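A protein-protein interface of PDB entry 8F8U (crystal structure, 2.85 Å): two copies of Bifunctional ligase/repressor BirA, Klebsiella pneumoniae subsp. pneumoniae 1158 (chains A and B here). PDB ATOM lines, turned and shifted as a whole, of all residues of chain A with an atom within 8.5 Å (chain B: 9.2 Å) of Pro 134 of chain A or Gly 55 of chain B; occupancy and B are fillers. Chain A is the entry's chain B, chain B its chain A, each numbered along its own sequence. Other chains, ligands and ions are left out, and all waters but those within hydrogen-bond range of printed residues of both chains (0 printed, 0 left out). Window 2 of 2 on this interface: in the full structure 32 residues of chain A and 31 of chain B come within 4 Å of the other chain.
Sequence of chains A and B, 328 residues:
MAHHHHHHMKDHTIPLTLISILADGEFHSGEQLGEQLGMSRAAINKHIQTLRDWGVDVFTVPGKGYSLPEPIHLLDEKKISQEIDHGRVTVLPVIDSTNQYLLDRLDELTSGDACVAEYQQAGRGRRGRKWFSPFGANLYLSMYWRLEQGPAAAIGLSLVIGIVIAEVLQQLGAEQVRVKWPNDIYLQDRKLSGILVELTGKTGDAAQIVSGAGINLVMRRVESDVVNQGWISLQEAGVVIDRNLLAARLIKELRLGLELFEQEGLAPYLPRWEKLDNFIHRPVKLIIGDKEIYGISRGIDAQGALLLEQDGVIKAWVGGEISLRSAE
O of Trp 54 of chain B sits close to OH of Tyr 119 of chain A (3.2 Å).
N of Phe 135 of chain A is in hydrogen-bond range of O of Trp 54 of chain B, 3.2 Å away.
The backbone NH (N) of Val 56 of chain B sits at hydrogen-bond distance from the backbone carbonyl oxygen (O) of Leu 51 of chain B, at 2.9 Å.
N of Tyr 119 of chain A lies within hydrogen-bond range of O of Pro 93 of chain A (3.0 Å).
Among the printed residues, pairs that only touch across the chains: Phe 135 of chain A with Val 56 of chain B (3.6 Å), Phe 135 of chain A with Ile 19 of chain B (3.7 Å), Pro 134 of chain A with Trp 54 of chain B (3.8 Å), Pro 134 of chain A with Gly 55 of chain B (3.8 Å) and Tyr 119 of chain A with Asp 53 of chain B (3.96 Å).
Printed residues of chain B within 4 Å of Tyr 119 of chain A: Asp 53 (3.96 Å) and Trp 54 (3.0 Å).
No residue of chain B comes within 4 Å of Ser 133 of chain A.
Of the printed residues of chain B, Pro 134 of chain A touches Trp 54 and Gly 55.
Printed residues of chain B within 4 Å of Phe 135 of chain A: Ile 19, Trp 54 and Val 56.
Printed residues of chain A within 4 Å of Ile 19 of chain B: Phe 135.
Of chain A, only Pro 134 comes within 4 Å of Gly 55 of chain B.
The nearest printed residue of chain A that does not touch Asp 53 of chain B is Pro 134 of chain A (7.2 Å).
Of the 15 printed residues of chain B, 5 touch a printed residue of chain A.
Hydrophobic or aromatic side chains of chain B within 4 Å of the printed part of chain A: Ile 19, Trp 54 and Val 56.
Of the 16 printed residues of chain A, 3 touch a printed residue of chain B.
Hydrophobic or aromatic side chains of chain A that line the printed part of chain B: Tyr 119, Pro 134 and Phe 135.
Along chain A the printed residues that touch a printed residue of chain B span positions 119 to 135.
Among the printed residues, 7 pairs touch across the chains.
No position is printed for both chains.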
ATOM      1  N   PRO A  93     -24.531  28.830   9.506  1.00  0.00           N
ATOM      2  CA  PRO A  93     -23.075  28.606   9.610  1.00  0.00           C
ATOM      3  C   PRO A  93     -22.670  27.154   9.430  1.00  0.00           C
ATOM      4  O   PRO A  93     -21.600  26.882   8.869  1.00  0.00           O
ATOM      5  CB  PRO A  93     -22.728  29.116  11.016  1.00  0.00           C
ATOM      6  CG  PRO A  93     -23.887  29.926  11.468  1.00  0.00           C
ATOM      7  CD  PRO A  93     -25.076  29.638  10.610  1.00  0.00           C
ATOM      8  N   GLU A 118     -20.374  28.580   6.601  1.00  0.00           N
ATOM      9  CA  GLU A 118     -18.926  28.465   6.735  1.00  0.00           C
ATOM     10  C   GLU A 118     -18.480  27.050   7.082  1.00  0.00           C
ATOM     11  O   GLU A 118     -17.319  26.856   7.465  1.00  0.00           O
ATOM     12  CB  GLU A 118     -18.378  29.464   7.766  1.00  0.00           C
ATOM     13  CG  GLU A 118     -18.997  29.415   9.147  1.00  0.00           C
ATOM     14  CD  GLU A 118     -18.415  30.477  10.066  1.00  0.00           C
ATOM     15  OE1 GLU A 118     -17.172  30.581  10.145  1.00  0.00           O
ATOM     16  OE2 GLU A 118     -19.196  31.213  10.707  1.00  0.00           O
ATOM     17  N   TYR A 119     -19.365  26.062   6.965  1.00  0.00           N
ATOM     18  CA  TYR A 119     -18.998  24.660   7.156  1.00  0.00           C
ATOM     19  C   TYR A 119     -20.032  23.808   6.444  1.00  0.00           C
ATOM     20  O   TYR A 119     -21.215  23.852   6.797  1.00  0.00           O
ATOM     21  CB  TYR A 119     -18.929  24.305   8.644  1.00  0.00           C
ATOM     22  CG  TYR A 119     -18.403  22.914   8.925  1.00  0.00           C
ATOM     23  CD1 TYR A 119     -17.097  22.566   8.606  1.00  0.00           C
ATOM     24  CD2 TYR A 119     -19.212  21.949   9.515  1.00  0.00           C
ATOM     25  CE1 TYR A 119     -16.612  21.298   8.863  1.00  0.00           C
ATOM     26  CE2 TYR A 119     -18.733  20.676   9.776  1.00  0.00           C
ATOM     27  CZ  TYR A 119     -17.432  20.358   9.447  1.00  0.00           C
ATOM     28  OH  TYR A 119     -16.949  19.095   9.704  1.00  0.00           O
ATOM     29  N   GLN A 120     -19.600  23.037   5.449  1.00  0.00           N
ATOM     30  CA  GLN A 120     -20.490  22.188   4.663  1.00  0.00           C
ATOM     31  C   GLN A 120     -20.229  20.738   5.051  1.00  0.00           C
ATOM     32  O   GLN A 120     -19.162  20.190   4.754  1.00  0.00           O
ATOM     33  CB  GLN A 120     -20.278  22.417   3.167  1.00  0.00           C
ATOM     34  CG  GLN A 120     -21.156  23.522   2.585  1.00  0.00           C
ATOM     35  CD  GLN A 120     -21.104  23.589   1.070  1.00  0.00           C
ATOM     36  OE1 GLN A 120     -22.074  23.977   0.420  1.00  0.00           O
ATOM     37  NE2 GLN A 120     -19.963  23.216   0.499  1.00  0.00           N
ATOM     38  N   SER A 133     -12.592  19.805   5.071  1.00  0.00           N
ATOM     39  CA  SER A 133     -12.474  21.254   5.201  1.00  0.00           C
ATOM     40  C   SER A 133     -13.124  21.725   6.499  1.00  0.00           C
ATOM     41  O   SER A 133     -14.344  21.654   6.650  1.00  0.00           O
ATOM     42  CB  SER A 133     -13.109  21.950   3.997  1.00  0.00           C
ATOM     43  OG  SER A 133     -12.842  21.235   2.801  1.00  0.00           O
ATOM     44  N   PRO A 134     -12.309  22.218   7.427  1.00  0.00           N
ATOM     45  CA  PRO A 134     -12.784  22.451   8.795  1.00  0.00           C
ATOM     46  C   PRO A 134     -13.673  23.686   8.900  1.00  0.00           C
ATOM     47  O   PRO A 134     -13.803  24.487   7.974  1.00  0.00           O
ATOM     48  CB  PRO A 134     -11.487  22.636   9.590  1.00  0.00           C
ATOM     49  CG  PRO A 134     -10.520  23.169   8.592  1.00  0.00           C
ATOM     50  CD  PRO A 134     -10.876  22.525   7.278  1.00  0.00           C
ATOM     51  N   PHE A 135     -14.288  23.819  10.075  1.00  0.00           N
ATOM     52  CA  PHE A 135     -15.213  24.912  10.346  1.00  0.00           C
ATOM     53  C   PHE A 135     -14.512  26.261  10.246  1.00  0.00           C
ATOM     54  O   PHE A 135     -13.381  26.429  10.714  1.00  0.00           O
ATOM     55  CB  PHE A 135     -15.831  24.737  11.735  1.00  0.00           C
ATOM     56  CG  PHE A 135     -16.763  25.849  12.139  1.00  0.00           C
ATOM     57  CD1 PHE A 135     -16.281  26.978  12.787  1.00  0.00           C
ATOM     58  CD2 PHE A 135     -18.121  25.760  11.883  1.00  0.00           C
ATOM     59  CE1 PHE A 135     -17.133  27.998  13.161  1.00  0.00           C
ATOM     60  CE2 PHE A 135     -18.978  26.777  12.257  1.00  0.00           C
ATOM     61  CZ  PHE A 135     -18.485  27.899  12.896  1.00  0.00           C
ATOM     62  N   GLY A 136     -15.195  27.228   9.634  1.00  0.00           N
ATOM     63  CA  GLY A 136     -14.678  28.571   9.484  1.00  0.00           C
ATOM     64  C   GLY A 136     -13.520  28.720   8.525  1.00  0.00           C
ATOM     65  O   GLY A 136     -13.093  29.853   8.271  1.00  0.00           O
ATOM     66  N   ALA A 137     -12.990  27.621   7.986  1.00  0.00           N
ATOM     67  CA  ALA A 137     -11.890  27.726   7.035  1.00  0.00           C
ATOM     68  C   ALA A 137     -12.348  28.301   5.703  1.00  0.00           C
ATOM     69  O   ALA A 137     -11.557  28.948   5.007  1.00  0.00           O
ATOM     70  CB  ALA A 137     -11.244  26.356   6.826  1.00  0.00           C
ATOM     71  N   ASN A 138     -13.606  28.080   5.336  1.00  0.00           N
ATOM     72  CA  ASN A 138     -14.119  28.476   4.034  1.00  0.00           C
ATOM     73  C   ASN A 138     -15.415  29.258   4.187  1.00  0.00           C
ATOM     74  O   ASN A 138     -16.166  29.068   5.148  1.00  0.00           O
ATOM     75  CB  ASN A 138     -14.374  27.257   3.129  1.00  0.00           C
ATOM     76  CG  ASN A 138     -13.098  26.544   2.724  1.00  0.00           C
ATOM     77  OD1 ASN A 138     -12.172  26.395   3.521  1.00  0.00           O
ATOM     78  ND2 ASN A 138     -13.043  26.097   1.475  1.00  0.00           N
ATOM     79  N   LEU A 139     -15.665  30.145   3.229  1.00  0.00           N
ATOM     80  CA  LEU A 139     -16.951  30.813   3.098  1.00  0.00           C
ATOM     81  C   LEU A 139     -17.730  30.119   1.991  1.00  0.00           C
ATOM     82  O   LEU A 139     -17.238  29.994   0.864  1.00  0.00           O
ATOM     83  CB  LEU A 139     -16.775  32.300   2.775  1.00  0.00           C
ATOM     84  CG  LEU A 139     -18.060  33.092   2.527  1.00  0.00           C
ATOM     85  CD1 LEU A 139     -18.979  33.021   3.737  1.00  0.00           C
ATOM     86  CD2 LEU A 139     -17.753  34.539   2.164  1.00  0.00           C
ATOM     87  N   TYR A 140     -18.939  29.669   2.310  1.00  0.00           N
ATOM     88  CA  TYR A 140     -19.776  28.927   1.377  1.00  0.00           C
ATOM     89  C   TYR A 140     -21.010  29.761   1.062  1.00  0.00           C
ATOM     90  O   TYR A 140     -21.771  30.118   1.967  1.00  0.00           O
ATOM     91  CB  TYR A 140     -20.172  27.571   1.963  1.00  0.00           C
ATOM     92  CG  TYR A 140     -19.026  26.602   2.127  1.00  0.00           C
ATOM     93  CD1 TYR A 140     -18.381  26.067   1.019  1.00  0.00           C
ATOM     94  CD2 TYR A 140     -18.595  26.211   3.390  1.00  0.00           C
ATOM     95  CE1 TYR A 140     -17.337  25.174   1.165  1.00  0.00           C
ATOM     96  CE2 TYR A 140     -17.550  25.320   3.545  1.00  0.00           C
ATOM     97  CZ  TYR A 140     -16.924  24.804   2.429  1.00  0.00           C
ATOM     98  OH  TYR A 140     -15.885  23.916   2.578  1.00  0.00           O
ATOM     99  N   ASN A 216     -11.649  29.658  -0.029  1.00  0.00           N
ATOM    100  CA  ASN A 216     -10.711  29.281   1.024  1.00  0.00           C
ATOM    101  C   ASN A 216     -10.250  30.548   1.735  1.00  0.00           C
ATOM    102  O   ASN A 216      -9.515  31.358   1.163  1.00  0.00           O
ATOM    103  CB  ASN A 216      -9.528  28.518   0.436  1.00  0.00           C
ATOM    104  CG  ASN A 216      -9.950  27.275  -0.324  1.00  0.00           C
ATOM    105  OD1 ASN A 216     -10.817  26.524   0.126  1.00  0.00           O
ATOM    106  ND2 ASN A 216      -9.341  27.055  -1.484  1.00  0.00           N
ATOM    107  N   VAL A 218      -8.961  30.689   5.249  1.00  0.00           N
ATOM    108  CA  VAL A 218      -7.783  30.518   6.139  1.00  0.00           C
ATOM    109  C   VAL A 218      -7.147  29.162   5.867  1.00  0.00           C
ATOM    110  O   VAL A 218      -7.733  28.374   5.106  1.00  0.00           O
ATOM    111  CB  VAL A 218      -8.189  30.653   7.617  1.00  0.00           C
ATOM    112  CG1 VAL A 218      -7.046  30.279   8.547  1.00  0.00           C
ATOM    113  CG2 VAL A 218      -8.693  32.050   7.933  1.00  0.00           C
ATOM    114  N   MET A 219      -5.986  28.917   6.462  1.00  0.00           N
ATOM    115  CA  MET A 219      -5.298  27.641   6.298  1.00  0.00           C
ATOM    116  C   MET A 219      -5.705  26.674   7.405  1.00  0.00           C
ATOM    117  O   MET A 219      -5.009  25.691   7.670  1.00  0.00           O
ATOM    118  CB  MET A 219      -3.774  27.814   6.304  1.00  0.00           C
ATOM    119  CG  MET A 219      -3.253  29.204   5.970  1.00  0.00           C
ATOM    120  SD  MET A 219      -1.457  29.244   6.159  1.00  0.00           S
ATOM    121  CE  MET A 219      -1.136  30.998   6.312  1.00  0.00           C
ATOM    122  N   ARG A 243     -15.200  37.846   6.949  1.00  0.00           N
ATOM    123  CA  ARG A 243     -16.055  36.959   6.166  1.00  0.00           C
ATOM    124  C   ARG A 243     -17.451  37.546   5.996  1.00  0.00           C
ATOM    125  O   ARG A 243     -18.052  37.428   4.920  1.00  0.00           O
ATOM    126  CB  ARG A 243     -16.120  35.576   6.811  1.00  0.00           C
ATOM    127  CG  ARG A 243     -16.498  35.572   8.276  1.00  0.00           C
ATOM    128  CD  ARG A 243     -16.326  34.183   8.859  1.00  0.00           C
ATOM    129  NE  ARG A 243     -14.922  33.854   9.063  1.00  0.00           N
ATOM    130  CZ  ARG A 243     -14.300  32.831   8.491  1.00  0.00           C
ATOM    131  NH1 ARG A 243     -14.938  31.996   7.687  1.00  0.00           N
ATOM    132  NH2 ARG A 243     -13.007  32.635   8.739  1.00  0.00           N
ATOM    133  N   ILE B  19     -19.303  28.120  20.518  1.00  0.00           N
ATOM    134  CA  ILE B  19     -18.130  28.644  19.822  1.00  0.00           C
ATOM    135  C   ILE B  19     -18.191  30.165  19.737  1.00  0.00           C
ATOM    136  O   ILE B  19     -17.153  30.838  19.798  1.00  0.00           O
ATOM    137  CB  ILE B  19     -17.977  27.988  18.431  1.00  0.00           C
ATOM    138  CG1 ILE B  19     -16.870  28.672  17.625  1.00  0.00           C
ATOM    139  CG2 ILE B  19     -19.284  28.007  17.669  1.00  0.00           C
ATOM    140  CD1 ILE B  19     -16.129  27.741  16.690  1.00  0.00           C
ATOM    141  N   ILE B  48     -18.504  20.787  22.980  1.00  0.00           N
ATOM    142  CA  ILE B  48     -17.122  21.082  22.617  1.00  0.00           C
ATOM    143  C   ILE B  48     -16.503  19.899  21.884  1.00  0.00           C
ATOM    144  O   ILE B  48     -15.601  20.073  21.053  1.00  0.00           O
ATOM    145  CB  ILE B  48     -16.338  21.500  23.878  1.00  0.00           C
ATOM    146  CG1 ILE B  48     -16.449  23.018  24.028  1.00  0.00           C
ATOM    147  CG2 ILE B  48     -14.883  21.047  23.819  1.00  0.00           C
ATOM    148  CD1 ILE B  48     -15.858  23.564  25.266  1.00  0.00           C
ATOM    149  N   GLN B  49     -17.006  18.688  22.137  1.00  0.00           N
ATOM    150  CA  GLN B  49     -16.609  17.541  21.331  1.00  0.00           C
ATOM    151  C   GLN B  49     -17.064  17.712  19.889  1.00  0.00           C
ATOM    152  O   GLN B  49     -16.279  17.531  18.952  1.00  0.00           O
ATOM    153  CB  GLN B  49     -17.183  16.254  21.923  1.00  0.00           C
ATOM    154  CG  GLN B  49     -16.246  15.075  21.813  1.00  0.00           C
ATOM    155  CD  GLN B  49     -14.822  15.457  22.142  1.00  0.00           C
ATOM    156  OE1 GLN B  49     -13.974  15.568  21.255  1.00  0.00           O
ATOM    157  NE2 GLN B  49     -14.549  15.664  23.426  1.00  0.00           N
ATOM    158  N   THR B  50     -18.343  18.053  19.691  1.00  0.00           N
ATOM    159  CA  THR B  50     -18.849  18.302  18.346  1.00  0.00           C
ATOM    160  C   THR B  50     -18.091  19.434  17.665  1.00  0.00           C
ATOM    161  O   THR B  50     -17.960  19.442  16.436  1.00  0.00           O
ATOM    162  CB  THR B  50     -20.345  18.615  18.388  1.00  0.00           C
ATOM    163  OG1 THR B  50     -20.557  19.877  19.032  1.00  0.00           O
ATOM    164  CG2 THR B  50     -21.094  17.529  19.144  1.00  0.00           C
ATOM    165  N   LEU B  51     -17.593  20.403  18.440  1.00  0.00           N
ATOM    166  CA  LEU B  51     -16.714  21.420  17.875  1.00  0.00           C
ATOM    167  C   LEU B  51     -15.446  20.787  17.315  1.00  0.00           C
ATOM    168  O   LEU B  51     -15.043  21.079  16.184  1.00  0.00           O
ATOM    169  CB  LEU B  51     -16.383  22.474  18.933  1.00  0.00           C
ATOM    170  CG  LEU B  51     -17.534  23.389  19.365  1.00  0.00           C
ATOM    171  CD1 LEU B  51     -17.004  24.712  19.896  1.00  0.00           C
ATOM    172  CD2 LEU B  51     -18.509  23.623  18.220  1.00  0.00           C
ATOM    173  N   ARG B  52     -14.806  19.914  18.096  1.00  0.00           N
ATOM    174  CA  ARG B  52     -13.657  19.173  17.581  1.00  0.00           C
ATOM    175  C   ARG B  52     -14.063  18.291  16.407  1.00  0.00           C
ATOM    176  O   ARG B  52     -13.284  18.100  15.466  1.00  0.00           O
ATOM    177  CB  ARG B  52     -13.034  18.327  18.693  1.00  0.00           C
ATOM    178  CG  ARG B  52     -12.204  19.126  19.675  1.00  0.00           C
ATOM    179  CD  ARG B  52     -11.363  18.253  20.591  1.00  0.00           C
ATOM    180  NE  ARG B  52     -11.776  18.385  21.982  1.00  0.00           N
ATOM    181  CZ  ARG B  52     -11.995  17.366  22.803  1.00  0.00           C
ATOM    182  NH1 ARG B  52     -11.803  16.115  22.417  1.00  0.00           N
ATOM    183  NH2 ARG B  52     -12.406  17.608  24.046  1.00  0.00           N
ATOM    184  N   ASP B  53     -15.281  17.748  16.448  1.00  0.00           N
ATOM    185  CA  ASP B  53     -15.780  16.948  15.334  1.00  0.00           C
ATOM    186  C   ASP B  53     -15.899  17.783  14.065  1.00  0.00           C
ATOM    187  O   ASP B  53     -15.604  17.304  12.965  1.00  0.00           O
ATOM    188  CB  ASP B  53     -17.123  16.318  15.703  1.00  0.00           C
ATOM    189  CG  ASP B  53     -16.977  15.192  16.711  1.00  0.00           C
ATOM    190  OD1 ASP B  53     -15.826  14.821  17.027  1.00  0.00           O
ATOM    191  OD2 ASP B  53     -18.011  14.677  17.188  1.00  0.00           O
ATOM    192  N   TRP B  54     -16.333  19.042  14.199  1.00  0.00           N
ATOM    193  CA  TRP B  54     -16.436  19.932  13.048  1.00  0.00           C
ATOM    194  C   TRP B  54     -15.078  20.349  12.500  1.00  0.00           C
ATOM    195  O   TRP B  54     -15.023  20.974  11.436  1.00  0.00           O
ATOM    196  CB  TRP B  54     -17.227  21.191  13.410  1.00  0.00           C
ATOM    197  CG  TRP B  54     -18.673  20.960  13.718  1.00  0.00           C
ATOM    198  CD1 TRP B  54     -19.401  19.834  13.462  1.00  0.00           C
ATOM    199  CD2 TRP B  54     -19.579  21.894  14.317  1.00  0.00           C
ATOM    200  NE1 TRP B  54     -20.699  20.005  13.878  1.00  0.00           N
ATOM    201  CE2 TRP B  54     -20.834  21.262  14.406  1.00  0.00           C
ATOM    202  CE3 TRP B  54     -19.446  23.203  14.793  1.00  0.00           C
ATOM    203  CZ2 TRP B  54     -21.950  21.893  14.949  1.00  0.00           C
ATOM    204  CZ3 TRP B  54     -20.554  23.827  15.332  1.00  0.00           C
ATOM    205  CH2 TRP B  54     -21.790  23.174  15.404  1.00  0.00           C
ATOM    206  N   GLY B  55     -13.992  20.036  13.200  1.00  0.00           N
ATOM    207  CA  GLY B  55     -12.667  20.471  12.817  1.00  0.00           C
ATOM    208  C   GLY B  55     -12.159  21.677  13.572  1.00  0.00           C
ATOM    209  O   GLY B  55     -11.044  22.135  13.297  1.00  0.00           O
ATOM    210  N   VAL B  56     -12.943  22.211  14.508  1.00  0.00           N
ATOM    211  CA  VAL B  56     -12.498  23.335  15.322  1.00  0.00           C
ATOM    212  C   VAL B  56     -11.411  22.846  16.271  1.00  0.00           C
ATOM    213  O   VAL B  56     -11.636  21.941  17.082  1.00  0.00           O
ATOM    214  CB  VAL B  56     -13.674  23.950  16.089  1.00  0.00           C
ATOM    215  CG1 VAL B  56     -13.190  25.042  17.001  1.00  0.00           C
ATOM    216  CG2 VAL B  56     -14.715  24.487  15.122  1.00  0.00           C
ATOM    217  N   ASP B  57     -10.224  23.445  16.175  1.00  0.00           N
ATOM    218  CA  ASP B  57      -9.091  23.032  17.001  1.00  0.00           C
ATOM    219  C   ASP B  57      -9.192  23.693  18.372  1.00  0.00           C
ATOM    220  O   ASP B  57      -8.511  24.674  18.684  1.00  0.00           O
ATOM    221  CB  ASP B  57      -7.780  23.377  16.307  1.00  0.00           C
ATOM    222  CG  ASP B  57      -7.033  22.151  15.828  1.00  0.00           C
ATOM    223  OD1 ASP B  57      -7.651  21.068  15.758  1.00  0.00           O
ATOM    224  OD2 ASP B  57      -5.837  22.270  15.504  1.00  0.00           O
ATOM    225  N   VAL B  58     -10.070  23.148  19.211  1.00  0.00           N
ATOM    226  CA  VAL B  58     -10.188  23.574  20.602  1.00  0.00           C
ATOM    227  C   VAL B  58      -9.366  22.635  21.481  1.00  0.00           C
ATOM    228  O   VAL B  58      -9.591  21.418  21.490  1.00  0.00           O
ATOM    229  CB  VAL B  58     -11.655  23.656  21.056  1.00  0.00           C
ATOM    230  CG1 VAL B  58     -12.394  22.356  20.813  1.00  0.00           C
ATOM    231  CG2 VAL B  58     -11.727  24.042  22.527  1.00  0.00           C
ATOM    232  N   PHE B  59      -8.385  23.194  22.183  1.00  0.00           N
ATOM    233  CA  PHE B  59      -7.479  22.444  23.046  1.00  0.00           C
ATOM    234  C   PHE B  59      -7.878  22.648  24.507  1.00  0.00           C
ATOM    235  O   PHE B  59      -8.099  23.785  24.938  1.00  0.00           O
ATOM    236  CB  PHE B  59      -6.029  22.855  22.804  1.00  0.00           C
ATOM    237  CG  PHE B  59      -5.359  22.060  21.720  1.00  0.00           C
ATOM    238  CD1 PHE B  59      -6.040  21.037  21.079  1.00  0.00           C
ATOM    239  CD2 PHE B  59      -4.059  22.336  21.335  1.00  0.00           C
ATOM    240  CE1 PHE B  59      -5.437  20.302  20.082  1.00  0.00           C
ATOM    241  CE2 PHE B  59      -3.449  21.601  20.339  1.00  0.00           C
ATOM    242  CZ  PHE B  59      -4.144  20.584  19.711  1.00  0.00           C
ATOM    243  N   LEU B  68      -9.539  28.427  21.913  1.00  0.00           N
ATOM    244  CA  LEU B  68      -9.178  28.490  20.503  1.00  0.00           C
ATOM    245  C   LEU B  68      -7.871  29.241  20.324  1.00  0.00           C
ATOM    246  O   LEU B  68      -7.699  30.322  20.901  1.00  0.00           O
ATOM    247  CB  LEU B  68     -10.270  29.173  19.677  1.00  0.00           C
ATOM    248  CG  LEU B  68     -11.679  28.597  19.668  1.00  0.00           C
ATOM    249  CD1 LEU B  68     -12.673  29.707  19.844  1.00  0.00           C
ATOM    250  CD2 LEU B  68     -11.913  27.914  18.354  1.00  0.00           C
ATOM    251  N   PRO B  69      -6.926  28.695  19.555  1.00  0.00           N
ATOM    252  CA  PRO B  69      -5.614  29.343  19.402  1.00  0.00           C
ATOM    253  C   PRO B  69      -5.679  30.774  18.877  1.00  0.00           C
ATOM    254  O   PRO B  69      -5.197  31.699  19.540  1.00  0.00           O
ATOM    255  CB  PRO B  69      -4.869  28.436  18.411  1.00  0.00           C
ATOM    256  CG  PRO B  69      -5.791  27.330  18.051  1.00  0.00           C
ATOM    257  CD  PRO B  69      -7.125  27.549  18.652  1.00  0.00           C
